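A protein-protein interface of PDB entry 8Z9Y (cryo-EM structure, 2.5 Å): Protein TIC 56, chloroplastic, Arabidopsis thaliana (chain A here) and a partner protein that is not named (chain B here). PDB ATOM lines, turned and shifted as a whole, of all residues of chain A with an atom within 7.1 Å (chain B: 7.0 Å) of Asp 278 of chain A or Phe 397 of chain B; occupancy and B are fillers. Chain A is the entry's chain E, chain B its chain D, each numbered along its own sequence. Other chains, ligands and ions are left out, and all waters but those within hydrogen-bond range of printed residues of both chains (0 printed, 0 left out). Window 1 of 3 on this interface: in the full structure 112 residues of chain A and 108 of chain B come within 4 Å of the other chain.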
ATOM      1  N   LYS A 242     -15.810  16.888  -8.921  1.00  0.00           N
ATOM      2  CA  LYS A 242     -15.825  15.953 -10.035  1.00  0.00           C
ATOM      3  C   LYS A 242     -17.015  15.012  -9.911  1.00  0.00           C
ATOM      4  O   LYS A 242     -17.314  14.514  -8.822  1.00  0.00           O
ATOM      5  CB  LYS A 242     -14.530  15.140 -10.090  1.00  0.00           C
ATOM      6  CG  LYS A 242     -13.268  15.974 -10.197  1.00  0.00           C
ATOM      7  CD  LYS A 242     -13.201  16.703 -11.525  1.00  0.00           C
ATOM      8  CE  LYS A 242     -11.790  16.699 -12.081  1.00  0.00           C
ATOM      9  NZ  LYS A 242     -11.630  17.668 -13.198  1.00  0.00           N
ATOM     10  N   SER A 248     -15.852  18.440 -14.523  1.00  0.00           N
ATOM     11  CA  SER A 248     -15.821  19.446 -13.471  1.00  0.00           C
ATOM     12  C   SER A 248     -17.163  20.163 -13.397  1.00  0.00           C
ATOM     13  O   SER A 248     -17.680  20.632 -14.416  1.00  0.00           O
ATOM     14  CB  SER A 248     -14.700  20.454 -13.720  1.00  0.00           C
ATOM     15  OG  SER A 248     -13.475  19.796 -13.988  1.00  0.00           O
ATOM     16  N   TRP A 273     -12.002  20.928  -5.190  1.00  0.00           N
ATOM     17  CA  TRP A 273     -10.872  21.837  -5.318  1.00  0.00           C
ATOM     18  C   TRP A 273     -11.263  23.213  -4.806  1.00  0.00           C
ATOM     19  O   TRP A 273     -12.333  23.729  -5.141  1.00  0.00           O
ATOM     20  CB  TRP A 273     -10.382  21.949  -6.762  1.00  0.00           C
ATOM     21  CG  TRP A 273      -9.140  22.771  -6.866  1.00  0.00           C
ATOM     22  CD1 TRP A 273      -7.860  22.347  -6.671  1.00  0.00           C
ATOM     23  CD2 TRP A 273      -9.059  24.169  -7.161  1.00  0.00           C
ATOM     24  NE1 TRP A 273      -6.985  23.390  -6.837  1.00  0.00           N
ATOM     25  CE2 TRP A 273      -7.697  24.521  -7.138  1.00  0.00           C
ATOM     26  CE3 TRP A 273     -10.006  25.156  -7.448  1.00  0.00           C
ATOM     27  CZ2 TRP A 273      -7.257  25.818  -7.390  1.00  0.00           C
ATOM     28  CZ3 TRP A 273      -9.567  26.443  -7.698  1.00  0.00           C
ATOM     29  CH2 TRP A 273      -8.206  26.763  -7.664  1.00  0.00           C
ATOM     30  N   GLY A 274     -10.383  23.807  -4.006  1.00  0.00           N
ATOM     31  CA  GLY A 274     -10.651  25.094  -3.398  1.00  0.00           C
ATOM     32  C   GLY A 274      -9.631  26.150  -3.762  1.00  0.00           C
ATOM     33  O   GLY A 274      -8.868  25.979  -4.715  1.00  0.00           O
ATOM     34  N   GLU A 275      -9.595  27.242  -2.999  1.00  0.00           N
ATOM     35  CA  GLU A 275      -8.761  28.379  -3.371  1.00  0.00           C
ATOM     36  C   GLU A 275      -7.278  28.049  -3.242  1.00  0.00           C
ATOM     37  O   GLU A 275      -6.535  28.082  -4.228  1.00  0.00           O
ATOM     38  CB  GLU A 275      -9.119  29.593  -2.511  1.00  0.00           C
ATOM     39  CG  GLU A 275      -8.523  30.925  -2.971  1.00  0.00           C
ATOM     40  CD  GLU A 275      -8.876  31.294  -4.404  1.00  0.00           C
ATOM     41  OE1 GLU A 275      -8.363  30.653  -5.346  1.00  0.00           O
ATOM     42  OE2 GLU A 275      -9.675  32.235  -4.588  1.00  0.00           O
ATOM     43  N   ASP A 276      -6.829  27.715  -2.033  1.00  0.00           N
ATOM     44  CA  ASP A 276      -5.406  27.627  -1.734  1.00  0.00           C
ATOM     45  C   ASP A 276      -4.910  26.191  -1.591  1.00  0.00           C
ATOM     46  O   ASP A 276      -3.939  25.945  -0.869  1.00  0.00           O
ATOM     47  CB  ASP A 276      -5.086  28.424  -0.470  1.00  0.00           C
ATOM     48  CG  ASP A 276      -3.813  29.230  -0.599  1.00  0.00           C
ATOM     49  OD1 ASP A 276      -3.515  29.691  -1.720  1.00  0.00           O
ATOM     50  OD2 ASP A 276      -3.112  29.406   0.418  1.00  0.00           O
ATOM     51  N   MET A 277      -5.549  25.236  -2.259  1.00  0.00           N
ATOM     52  CA  MET A 277      -5.080  23.859  -2.257  1.00  0.00           C
ATOM     53  C   MET A 277      -4.365  23.546  -3.564  1.00  0.00           C
ATOM     54  O   MET A 277      -4.638  24.151  -4.605  1.00  0.00           O
ATOM     55  CB  MET A 277      -6.226  22.869  -2.036  1.00  0.00           C
ATOM     56  CG  MET A 277      -7.128  23.214  -0.867  1.00  0.00           C
ATOM     57  SD  MET A 277      -8.362  21.941  -0.545  1.00  0.00           S
ATOM     58  CE  MET A 277      -8.877  21.535  -2.207  1.00  0.00           C
ATOM     59  N   ASP A 278      -3.441  22.589  -3.496  1.00  0.00           N
ATOM     60  CA  ASP A 278      -2.590  22.250  -4.625  1.00  0.00           C
ATOM     61  C   ASP A 278      -3.153  21.132  -5.491  1.00  0.00           C
ATOM     62  O   ASP A 278      -2.800  21.045  -6.672  1.00  0.00           O
ATOM     63  CB  ASP A 278      -1.199  21.851  -4.123  1.00  0.00           C
ATOM     64  CG  ASP A 278      -0.205  21.668  -5.246  1.00  0.00           C
ATOM     65  OD1 ASP A 278      -0.322  22.386  -6.260  1.00  0.00           O
ATOM     66  OD2 ASP A 278       0.692  20.810  -5.115  1.00  0.00           O
ATOM     67  N   GLU A 279      -4.019  20.284  -4.943  1.00  0.00           N
ATOM     68  CA  GLU A 279      -4.554  19.157  -5.690  1.00  0.00           C
ATOM     69  C   GLU A 279      -5.953  18.842  -5.181  1.00  0.00           C
ATOM     70  O   GLU A 279      -6.347  19.258  -4.089  1.00  0.00           O
ATOM     71  CB  GLU A 279      -3.652  17.924  -5.570  1.00  0.00           C
ATOM     72  CG  GLU A 279      -3.520  17.396  -4.152  1.00  0.00           C
ATOM     73  CD  GLU A 279      -2.564  16.225  -4.052  1.00  0.00           C
ATOM     74  OE1 GLU A 279      -1.372  16.399  -4.381  1.00  0.00           O
ATOM     75  OE2 GLU A 279      -3.003  15.130  -3.644  1.00  0.00           O
ATOM     76  N   TRP A 280      -6.700  18.105  -5.995  1.00  0.00           N
ATOM     77  CA  TRP A 280      -8.051  17.714  -5.621  1.00  0.00           C
ATOM     78  C   TRP A 280      -8.011  16.698  -4.487  1.00  0.00           C
ATOM     79  O   TRP A 280      -7.171  15.797  -4.469  1.00  0.00           O
ATOM     80  CB  TRP A 280      -8.787  17.135  -6.828  1.00  0.00           C
ATOM     81  CG  TRP A 280      -8.928  18.104  -7.960  1.00  0.00           C
ATOM     82  CD1 TRP A 280      -7.924  18.631  -8.718  1.00  0.00           C
ATOM     83  CD2 TRP A 280     -10.145  18.666  -8.461  1.00  0.00           C
ATOM     84  NE1 TRP A 280      -8.440  19.485  -9.660  1.00  0.00           N
ATOM     85  CE2 TRP A 280      -9.802  19.524  -9.523  1.00  0.00           C
ATOM     86  CE3 TRP A 280     -11.492  18.528  -8.115  1.00  0.00           C
ATOM     87  CZ2 TRP A 280     -10.756  20.239 -10.242  1.00  0.00           C
ATOM     88  CZ3 TRP A 280     -12.436  19.237  -8.828  1.00  0.00           C
ATOM     89  CH2 TRP A 280     -12.065  20.082  -9.880  1.00  0.00           C
ATOM     90  N   ALA A 368      -9.281  10.216 -14.294  1.00  0.00           N
ATOM     91  CA  ALA A 368      -8.541  11.464 -14.149  1.00  0.00           C
ATOM     92  C   ALA A 368      -8.539  12.291 -15.428  1.00  0.00           C
ATOM     93  O   ALA A 368      -8.293  13.499 -15.368  1.00  0.00           O
ATOM     94  CB  ALA A 368      -7.105  11.176 -13.714  1.00  0.00           C
ATOM     95  N   SER A 371     -12.422  14.918 -18.280  1.00  0.00           N
ATOM     96  CA  SER A 371     -12.769  16.189 -18.903  1.00  0.00           C
ATOM     97  C   SER A 371     -12.375  16.261 -20.372  1.00  0.00           C
ATOM     98  O   SER A 371     -12.801  17.194 -21.061  1.00  0.00           O
ATOM     99  CB  SER A 371     -12.116  17.340 -18.137  1.00  0.00           C
ATOM    100  OG  SER A 371     -10.794  17.011 -17.751  1.00  0.00           O
ATOM    101  N   LEU B 206      -3.302  30.566  -4.539  1.00  0.00           N
ATOM    102  CA  LEU B 206      -3.231  29.776  -5.760  1.00  0.00           C
ATOM    103  C   LEU B 206      -4.528  29.919  -6.545  1.00  0.00           C
ATOM    104  O   LEU B 206      -5.619  29.948  -5.972  1.00  0.00           O
ATOM    105  CB  LEU B 206      -2.976  28.306  -5.430  1.00  0.00           C
ATOM    106  CG  LEU B 206      -1.557  27.920  -5.012  1.00  0.00           C
ATOM    107  CD1 LEU B 206      -1.487  26.441  -4.677  1.00  0.00           C
ATOM    108  CD2 LEU B 206      -0.563  28.266  -6.103  1.00  0.00           C
ATOM    109  N   TRP B 208      -6.654  28.552 -10.127  1.00  0.00           N
ATOM    110  CA  TRP B 208      -6.786  27.667 -11.277  1.00  0.00           C
ATOM    111  C   TRP B 208      -7.114  28.508 -12.504  1.00  0.00           C
ATOM    112  O   TRP B 208      -8.164  29.156 -12.555  1.00  0.00           O
ATOM    113  CB  TRP B 208      -7.874  26.626 -11.024  1.00  0.00           C
ATOM    114  CG  TRP B 208      -8.107  25.667 -12.152  1.00  0.00           C
ATOM    115  CD1 TRP B 208      -7.293  25.439 -13.221  1.00  0.00           C
ATOM    116  CD2 TRP B 208      -9.237  24.804 -12.317  1.00  0.00           C
ATOM    117  NE1 TRP B 208      -7.846  24.488 -14.042  1.00  0.00           N
ATOM    118  CE2 TRP B 208      -9.040  24.082 -13.509  1.00  0.00           C
ATOM    119  CE3 TRP B 208     -10.397  24.573 -11.573  1.00  0.00           C
ATOM    120  CZ2 TRP B 208      -9.958  23.145 -13.973  1.00  0.00           C
ATOM    121  CZ3 TRP B 208     -11.307  23.642 -12.035  1.00  0.00           C
ATOM    122  CH2 TRP B 208     -11.083  22.941 -13.224  1.00  0.00           C
ATOM    123  N   VAL B 209      -6.218  28.499 -13.491  1.00  0.00           N
ATOM    124  CA  VAL B 209      -6.343  29.347 -14.665  1.00  0.00           C
ATOM    125  C   VAL B 209      -6.298  28.482 -15.917  1.00  0.00           C
ATOM    126  O   VAL B 209      -5.998  27.290 -15.873  1.00  0.00           O
ATOM    127  CB  VAL B 209      -5.245  30.428 -14.725  1.00  0.00           C
ATOM    128  CG1 VAL B 209      -5.336  31.345 -13.521  1.00  0.00           C
ATOM    129  CG2 VAL B 209      -3.875  29.782 -14.805  1.00  0.00           C
ATOM    130  N   SER B 210      -6.609  29.115 -17.047  1.00  0.00           N
ATOM    131  CA  SER B 210      -6.558  28.464 -18.354  1.00  0.00           C
ATOM    132  C   SER B 210      -6.290  29.566 -19.375  1.00  0.00           C
ATOM    133  O   SER B 210      -7.203  30.312 -19.737  1.00  0.00           O
ATOM    134  CB  SER B 210      -7.851  27.719 -18.651  1.00  0.00           C
ATOM    135  OG  SER B 210      -7.748  26.972 -19.848  1.00  0.00           O
ATOM    136  N   TYR B 219      -1.575  26.988 -21.082  1.00  0.00           N
ATOM    137  CA  TYR B 219      -1.273  26.435 -19.771  1.00  0.00           C
ATOM    138  C   TYR B 219      -2.567  26.280 -18.988  1.00  0.00           C
ATOM    139  O   TYR B 219      -3.412  27.179 -18.990  1.00  0.00           O
ATOM    140  CB  TYR B 219      -0.287  27.322 -19.000  1.00  0.00           C
ATOM    141  CG  TYR B 219      -0.063  26.889 -17.568  1.00  0.00           C
ATOM    142  CD1 TYR B 219       0.877  25.916 -17.256  1.00  0.00           C
ATOM    143  CD2 TYR B 219      -0.786  27.456 -16.529  1.00  0.00           C
ATOM    144  CE1 TYR B 219       1.084  25.517 -15.951  1.00  0.00           C
ATOM    145  CE2 TYR B 219      -0.586  27.061 -15.222  1.00  0.00           C
ATOM    146  CZ  TYR B 219       0.350  26.094 -14.939  1.00  0.00           C
ATOM    147  OH  TYR B 219       0.551  25.703 -13.637  1.00  0.00           O
ATOM    148  N   GLU B 220      -2.714  25.138 -18.319  1.00  0.00           N
ATOM    149  CA  GLU B 220      -3.877  24.852 -17.485  1.00  0.00           C
ATOM    150  C   GLU B 220      -3.386  24.299 -16.155  1.00  0.00           C
ATOM    151  O   GLU B 220      -2.804  23.211 -16.109  1.00  0.00           O
ATOM    152  CB  GLU B 220      -4.818  23.863 -18.167  1.00  0.00           C
ATOM    153  CG  GLU B 220      -5.858  24.513 -19.054  1.00  0.00           C
ATOM    154  CD  GLU B 220      -6.421  23.558 -20.085  1.00  0.00           C
ATOM    155  OE1 GLU B 220      -5.625  22.924 -20.808  1.00  0.00           O
ATOM    156  OE2 GLU B 220      -7.661  23.447 -20.177  1.00  0.00           O
ATOM    157  N   GLY B 221      -3.625  25.037 -15.081  1.00  0.00           N
ATOM    158  CA  GLY B 221      -3.194  24.606 -13.769  1.00  0.00           C
ATOM    159  C   GLY B 221      -3.211  25.766 -12.794  1.00  0.00           C
ATOM    160  O   GLY B 221      -3.792  26.818 -13.058  1.00  0.00           O
ATOM    161  N   THR B 222      -2.557  25.543 -11.660  1.00  0.00           N
ATOM    162  CA  THR B 222      -2.493  26.535 -10.599  1.00  0.00           C
ATOM    163  C   THR B 222      -1.331  27.492 -10.831  1.00  0.00           C
ATOM    164  O   THR B 222      -0.293  27.119 -11.384  1.00  0.00           O
ATOM    165  CB  THR B 222      -2.345  25.862  -9.234  1.00  0.00           C
ATOM    166  OG1 THR B 222      -1.216  24.980  -9.255  1.00  0.00           O
ATOM    167  CG2 THR B 222      -3.593  25.064  -8.898  1.00  0.00           C
ATOM    168  N   GLN B 229       2.758  27.497 -10.429  1.00  0.00           N
ATOM    169  CA  GLN B 229       3.123  26.828  -9.191  1.00  0.00           C
ATOM    170  C   GLN B 229       2.188  25.652  -8.963  1.00  0.00           C
ATOM    171  O   GLN B 229       0.980  25.759  -9.190  1.00  0.00           O
ATOM    172  CB  GLN B 229       3.061  27.783  -7.993  1.00  0.00           C
ATOM    173  CG  GLN B 229       4.273  28.686  -7.857  1.00  0.00           C
ATOM    174  CD  GLN B 229       5.211  28.232  -6.759  1.00  0.00           C
ATOM    175  OE1 GLN B 229       4.880  27.347  -5.973  1.00  0.00           O
ATOM    176  NE2 GLN B 229       6.388  28.838  -6.702  1.00  0.00           N
ATOM    177  N   GLY B 230       2.749  24.536  -8.508  1.00  0.00           N
ATOM    178  CA  GLY B 230       1.963  23.339  -8.294  1.00  0.00           C
ATOM    179  C   GLY B 230       1.824  22.502  -9.548  1.00  0.00           C
ATOM    180  O   GLY B 230       2.759  22.418 -10.348  1.00  0.00           O
ATOM    181  N   LYS B 231       0.661  21.888  -9.737  1.00  0.00           N
ATOM    182  CA  LYS B 231       0.423  21.026 -10.885  1.00  0.00           C
ATOM    183  C   LYS B 231      -0.160  21.824 -12.041  1.00  0.00           C
ATOM    184  O   LYS B 231      -0.955  22.746 -11.838  1.00  0.00           O
ATOM    185  CB  LYS B 231      -0.520  19.882 -10.512  1.00  0.00           C
ATOM    186  CG  LYS B 231      -0.315  19.342  -9.111  1.00  0.00           C
ATOM    187  CD  LYS B 231       0.454  18.035  -9.135  1.00  0.00           C
ATOM    188  CE  LYS B 231       0.900  17.636  -7.741  1.00  0.00           C
ATOM    189  NZ  LYS B 231      -0.221  17.699  -6.765  1.00  0.00           N
ATOM    190  N   GLY B 232       0.239  21.462 -13.254  1.00  0.00           N
ATOM    191  CA  GLY B 232      -0.251  22.141 -14.437  1.00  0.00           C
ATOM    192  C   GLY B 232       0.189  21.425 -15.692  1.00  0.00           C
ATOM    193  O   GLY B 232       1.093  20.583 -15.667  1.00  0.00           O
ATOM    194  N   VAL B 233      -0.464  21.777 -16.796  1.00  0.00           N
ATOM    195  CA  VAL B 233      -0.206  21.177 -18.099  1.00  0.00           C
ATOM    196  C   VAL B 233       0.196  22.281 -19.065  1.00  0.00           C
ATOM    197  O   VAL B 233      -0.496  23.301 -19.169  1.00  0.00           O
ATOM    198  CB  VAL B 233      -1.435  20.412 -18.624  1.00  0.00           C
ATOM    199  CG1 VAL B 233      -1.188  19.912 -20.035  1.00  0.00           C
ATOM    200  CG2 VAL B 233      -1.775  19.261 -17.696  1.00  0.00           C
ATOM    201  N   GLU B 246       4.657  18.878 -11.867  1.00  0.00           N
ATOM    202  CA  GLU B 246       4.716  19.925 -10.860  1.00  0.00           C
ATOM    203  C   GLU B 246       5.583  21.086 -11.329  1.00  0.00           C
ATOM    204  O   GLU B 246       6.530  20.912 -12.101  1.00  0.00           O
ATOM    205  CB  GLU B 246       5.254  19.367  -9.543  1.00  0.00           C
ATOM    206  CG  GLU B 246       4.381  18.283  -8.936  1.00  0.00           C
ATOM    207  CD  GLU B 246       5.169  17.302  -8.093  1.00  0.00           C
ATOM    208  OE1 GLU B 246       6.339  17.597  -7.772  1.00  0.00           O
ATOM    209  OE2 GLU B 246       4.618  16.235  -7.751  1.00  0.00           O
ATOM    210  N   TRP B 247       5.248  22.281 -10.850  1.00  0.00           N
ATOM    211  CA  TRP B 247       5.958  23.500 -11.205  1.00  0.00           C
ATOM    212  C   TRP B 247       6.402  24.224  -9.943  1.00  0.00           C
ATOM    213  O   TRP B 247       5.882  23.989  -8.850  1.00  0.00           O
ATOM    214  CB  TRP B 247       5.088  24.436 -12.055  1.00  0.00           C
ATOM    215  CG  TRP B 247       4.631  23.846 -13.350  1.00  0.00           C
ATOM    216  CD1 TRP B 247       3.652  22.914 -13.524  1.00  0.00           C
ATOM    217  CD2 TRP B 247       5.125  24.158 -14.656  1.00  0.00           C
ATOM    218  NE1 TRP B 247       3.511  22.621 -14.858  1.00  0.00           N
ATOM    219  CE2 TRP B 247       4.403  23.373 -15.574  1.00  0.00           C
ATOM    220  CE3 TRP B 247       6.110  25.024 -15.138  1.00  0.00           C
ATOM    221  CZ2 TRP B 247       4.635  23.428 -16.945  1.00  0.00           C
ATOM    222  CZ3 TRP B 247       6.339  25.076 -16.499  1.00  0.00           C
ATOM    223  CH2 TRP B 247       5.605  24.283 -17.387  1.00  0.00           C
ATOM    224  N   ALA B 392      -0.741  12.339 -13.882  1.00  0.00           N
ATOM    225  CA  ALA B 392      -2.166  12.044 -13.776  1.00  0.00           C
ATOM    226  C   ALA B 392      -2.868  13.046 -12.869  1.00  0.00           C
ATOM    227  O   ALA B 392      -3.989  13.479 -13.157  1.00  0.00           O
ATOM    228  CB  ALA B 392      -2.373  10.620 -13.265  1.00  0.00           C
ATOM    229  N   LYS B 393      -2.224  13.419 -11.761  1.00  0.00           N
ATOM    230  CA  LYS B 393      -2.788  14.440 -10.882  1.00  0.00           C
ATOM    231  C   LYS B 393      -2.908  15.779 -11.597  1.00  0.00           C
ATOM    232  O   LYS B 393      -3.912  16.485 -11.447  1.00  0.00           O
ATOM    233  CB  LYS B 393      -1.927  14.588  -9.629  1.00  0.00           C
ATOM    234  CG  LYS B 393      -2.311  13.674  -8.481  1.00  0.00           C
ATOM    235  CD  LYS B 393      -1.222  13.659  -7.423  1.00  0.00           C
ATOM    236  CE  LYS B 393      -1.593  12.767  -6.254  1.00  0.00           C
ATOM    237  NZ  LYS B 393      -0.748  13.050  -5.063  1.00  0.00           N
ATOM    238  N   ALA B 394      -1.889  16.149 -12.375  1.00  0.00           N
ATOM    239  CA  ALA B 394      -1.903  17.440 -13.054  1.00  0.00           C
ATOM    240  C   ALA B 394      -2.927  17.478 -14.179  1.00  0.00           C
ATOM    241  O   ALA B 394      -3.428  18.555 -14.520  1.00  0.00           O
ATOM    242  CB  ALA B 394      -0.512  17.763 -13.595  1.00  0.00           C
ATOM    243  N   ARG B 395      -3.248  16.325 -14.768  1.00  0.00           N
ATOM    244  CA  ARG B 395      -4.235  16.291 -15.842  1.00  0.00           C
ATOM    245  C   ARG B 395      -5.642  16.644 -15.377  1.00  0.00           C
ATOM    246  O   ARG B 395      -6.508  16.885 -16.223  1.00  0.00           O
ATOM    247  CB  ARG B 395      -4.252  14.914 -16.505  1.00  0.00           C
ATOM    248  CG  ARG B 395      -3.150  14.707 -17.525  1.00  0.00           C
ATOM    249  CD  ARG B 395      -3.675  13.988 -18.754  1.00  0.00           C
ATOM    250  NE  ARG B 395      -3.947  12.579 -18.496  1.00  0.00           N
ATOM    251  CZ  ARG B 395      -3.016  11.639 -18.408  1.00  0.00           C
ATOM    252  NH1 ARG B 395      -1.733  11.921 -18.560  1.00  0.00           N
ATOM    253  NH2 ARG B 395      -3.383  10.385 -18.167  1.00  0.00           N
ATOM    254  N   MET B 396      -5.895  16.677 -14.068  1.00  0.00           N
ATOM    255  CA  MET B 396      -7.222  17.013 -13.567  1.00  0.00           C
ATOM    256  C   MET B 396      -7.568  18.488 -13.735  1.00  0.00           C
ATOM    257  O   MET B 396      -8.725  18.859 -13.512  1.00  0.00           O
ATOM    258  CB  MET B 396      -7.345  16.622 -12.095  1.00  0.00           C
ATOM    259  CG  MET B 396      -7.874  15.216 -11.872  1.00  0.00           C
ATOM    260  SD  MET B 396      -8.001  14.788 -10.126  1.00  0.00           S
ATOM    261  CE  MET B 396      -6.555  13.756  -9.925  1.00  0.00           C
ATOM    262  N   PHE B 397      -6.611  19.329 -14.115  1.00  0.00           N
ATOM    263  CA  PHE B 397      -6.844  20.756 -14.289  1.00  0.00           C
ATOM    264  C   PHE B 397      -7.080  21.140 -15.743  1.00  0.00           C
ATOM    265  O   PHE B 397      -7.119  22.333 -16.060  1.00  0.00           O
ATOM    266  CB  PHE B 397      -5.668  21.555 -13.724  1.00  0.00           C
ATOM    267  CG  PHE B 397      -5.569  21.511 -12.228  1.00  0.00           C
ATOM    268  CD1 PHE B 397      -6.491  22.176 -11.441  1.00  0.00           C
ATOM    269  CD2 PHE B 397      -4.554  20.806 -11.609  1.00  0.00           C
ATOM    270  CE1 PHE B 397      -6.403  22.137 -10.064  1.00  0.00           C
ATOM    271  CE2 PHE B 397      -4.460  20.764 -10.233  1.00  0.00           C
ATOM    272  CZ  PHE B 397      -5.387  21.430  -9.460  1.00  0.00           C
ATOM    273  N   VAL B 398      -7.236  20.169 -16.625  1.00  0.00           N
ATOM    274  CA  VAL B 398      -7.409  20.419 -18.051  1.00  0.00           C
ATOM    275  C   VAL B 398      -8.879  20.698 -18.338  1.00  0.00           C
ATOM    276  O   VAL B 398      -9.776  20.134 -17.701  1.00  0.00           O
ATOM    277  CB  VAL B 398      -6.881  19.226 -18.877  1.00  0.00           C
ATOM    278  CG1 VAL B 398      -7.039  19.480 -20.366  1.00  0.00           C
ATOM    279  CG2 VAL B 398      -5.427  18.958 -18.538  1.00  0.00           C
ATOM    280  N   ASN B 399      -9.122  21.592 -19.299  1.00  0.00           N
ATOM    281  CA  ASN B 399     -10.464  21.928 -19.776  1.00  0.00           C
ATOM    282  C   ASN B 399     -11.308  22.560 -18.667  1.00  0.00           C
ATOM    283  O   ASN B 399     -12.377  22.069 -18.299  1.00  0.00           O
ATOM    284  CB  ASN B 399     -11.162  20.700 -20.369  1.00  0.00           C
ATOM    285  CG  ASN B 399     -10.804  20.475 -21.823  1.00  0.00           C
ATOM    286  OD1 ASN B 399     -10.117  21.290 -22.437  1.00  0.00           O
ATOM    287  ND2 ASN B 399     -11.269  19.366 -22.382  1.00  0.00           N
ATOM    288  N   LYS B 400     -10.802  23.663 -18.134  1.00  0.00           N
ATOM    289  CA  LYS B 400     -11.569  24.436 -17.168  1.00  0.00           C
ATOM    290  C   LYS B 400     -12.773  25.062 -17.864  1.00  0.00           C
ATOM    291  O   LYS B 400     -12.614  25.692 -18.915  1.00  0.00           O
ATOM    292  CB  LYS B 400     -10.701  25.513 -16.529  1.00  0.00           C
ATOM    293  CG  LYS B 400     -11.453  26.416 -15.572  1.00  0.00           C
ATOM    294  CD  LYS B 400     -10.521  27.405 -14.900  1.00  0.00           C
ATOM    295  CE  LYS B 400     -11.185  28.048 -13.698  1.00  0.00           C
ATOM    296  NZ  LYS B 400     -10.553  29.346 -13.347  1.00  0.00           N
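The indole nitrogen of Trp 208 of chain B lies within hydrogen-bond range of the backbone carbonyl oxygen of Phe 397 of chain B (3.0 Å). NZ of Lys 400 of chain B is in hydrogen-bond range of O of Trp 208 of chain B. N of Asn 399 of chain B is in hydrogen-bond range of OE2 of Glu 220 of chain B (2.5 Å). The backbone NH of Thr 222 of chain B sits at hydrogen-bond distance from the backbone carbonyl oxygen of Lys 231 of chain B, 3.2 Å away. The backbone NH (N) of Trp 247 of chain B is in hydrogen-bond range of the backbone carbonyl oxygen (O) of Gly 230 of chain B, 2.5 Å away. NE1 of Trp 273 of chain A sits at hydrogen-bond distance from O of Met 277 of chain A, at 3.3 Å.
Among the printed residues, pairs that only touch across the chains: Trp 273 of chain A with Trp 208 of chain B (3.4 Å), Trp 273 of chain A with Phe 397 of chain B (3.5 Å), Met 277 of chain A with Leu 206 of chain B (3.9 Å), Asp 278 of chain A with Gly 230 of chain B (3.2 Å), Asp 278 of chain A with Phe 397 of chain B (3.8 Å), Trp 280 of chain A with Trp 208 of chain B (3.9 Å), Trp 280 of chain A with Met 396 of chain B (3.9 Å), Trp 280 of chain A with Phe 397 of chain B (3.4 Å), Ala 368 of chain A with Ala 392 of chain B (3.9 Å), Ala 368 of chain A with Arg 395 of chain B (3.9 Å) and Ala 368 of chain A with Met 396 of chain B (3.9 Å).
The backbone carbonyl oxygen of Glu 275 of chain A lies close to the backbone carbonyl oxygen of Leu 206 of chain B, 2.7 Å away. The backbone NH (N) of Leu 206 of chain B sits at hydrogen-bond distance from the side-chain carboxylate (OD1) of Asp 276 of chain A, 3.0 Å away. The side-chain amino group of Lys 231 of chain B lies within salt-bridge range of the side-chain carboxylate of Asp 278 of chain A. The side-chain amino group (NZ) of Lys 231 of chain B lies within salt-bridge range of the side-chain carboxylate (OE1) of Glu 279 of chain A, at 2.9 Å. The side-chain amino group (NZ) of Lys 393 of chain B is in salt-bridge range of the side-chain carboxylate (OE2) of Glu 279 of chain A (3.4 Å). O of Met 396 of chain B lies within hydrogen-bond range of NZ of Lys 242 of chain A (3.2 Å). The backbone carbonyl oxygen of Val 398 of chain B lies within hydrogen-bond range of the side-chain hydroxyl of Ser 371 of chain A (3.3 Å). O of Ser 371 of chain A is in hydrogen-bond range of ND2 of Asn 399 of chain B (3.0 Å).
Of the 12 printed residues of chain A, 10 touch a printed residue of chain B. Hydrophobic or aromatic side chains of chain A that line the printed part of chain B: Trp 273, Trp 280 and Ala 368. Among the printed residues, 19 pairs touch across the chains. Among the printed residues, Asp or Glu carboxylates within 4 Å of a Lys or Arg side-chain nitrogen of the other chain: Asp 278 of chain A with Lys 231 of chain B, Glu 279 of chain A with Lys 231 of chain B and Glu 279 of chain A with Lys 393 of chain B.
Printed residues of chain B within 4 Å of Trp 273 of chain A: Trp 208 and Phe 397. Printed residues of chain B within 4 Å of Asp 278 of chain A: Gly 230, Lys 231 and Phe 397. Printed residues of chain B within 4 Å of Ala 368 of chain A: Ala 392, Arg 395 and Met 396. Of the printed residues of chain A, Ala 392 of chain B touches Ala 368 (3.9 Å). Of the printed residues of chain A, Arg 395 of chain B touches Ala 368 (3.9 Å). Phe 397 of chain B touches just these residues of chain A: Trp 273, Asp 278 and Trp 280. Of the printed residues of chain A, Val 398 of chain B touches Ser 371 (3.3 Å). The nearest printed residue of chain B that does not touch Trp 273 of chain A is Thr 222 of chain B (4.03 Å).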
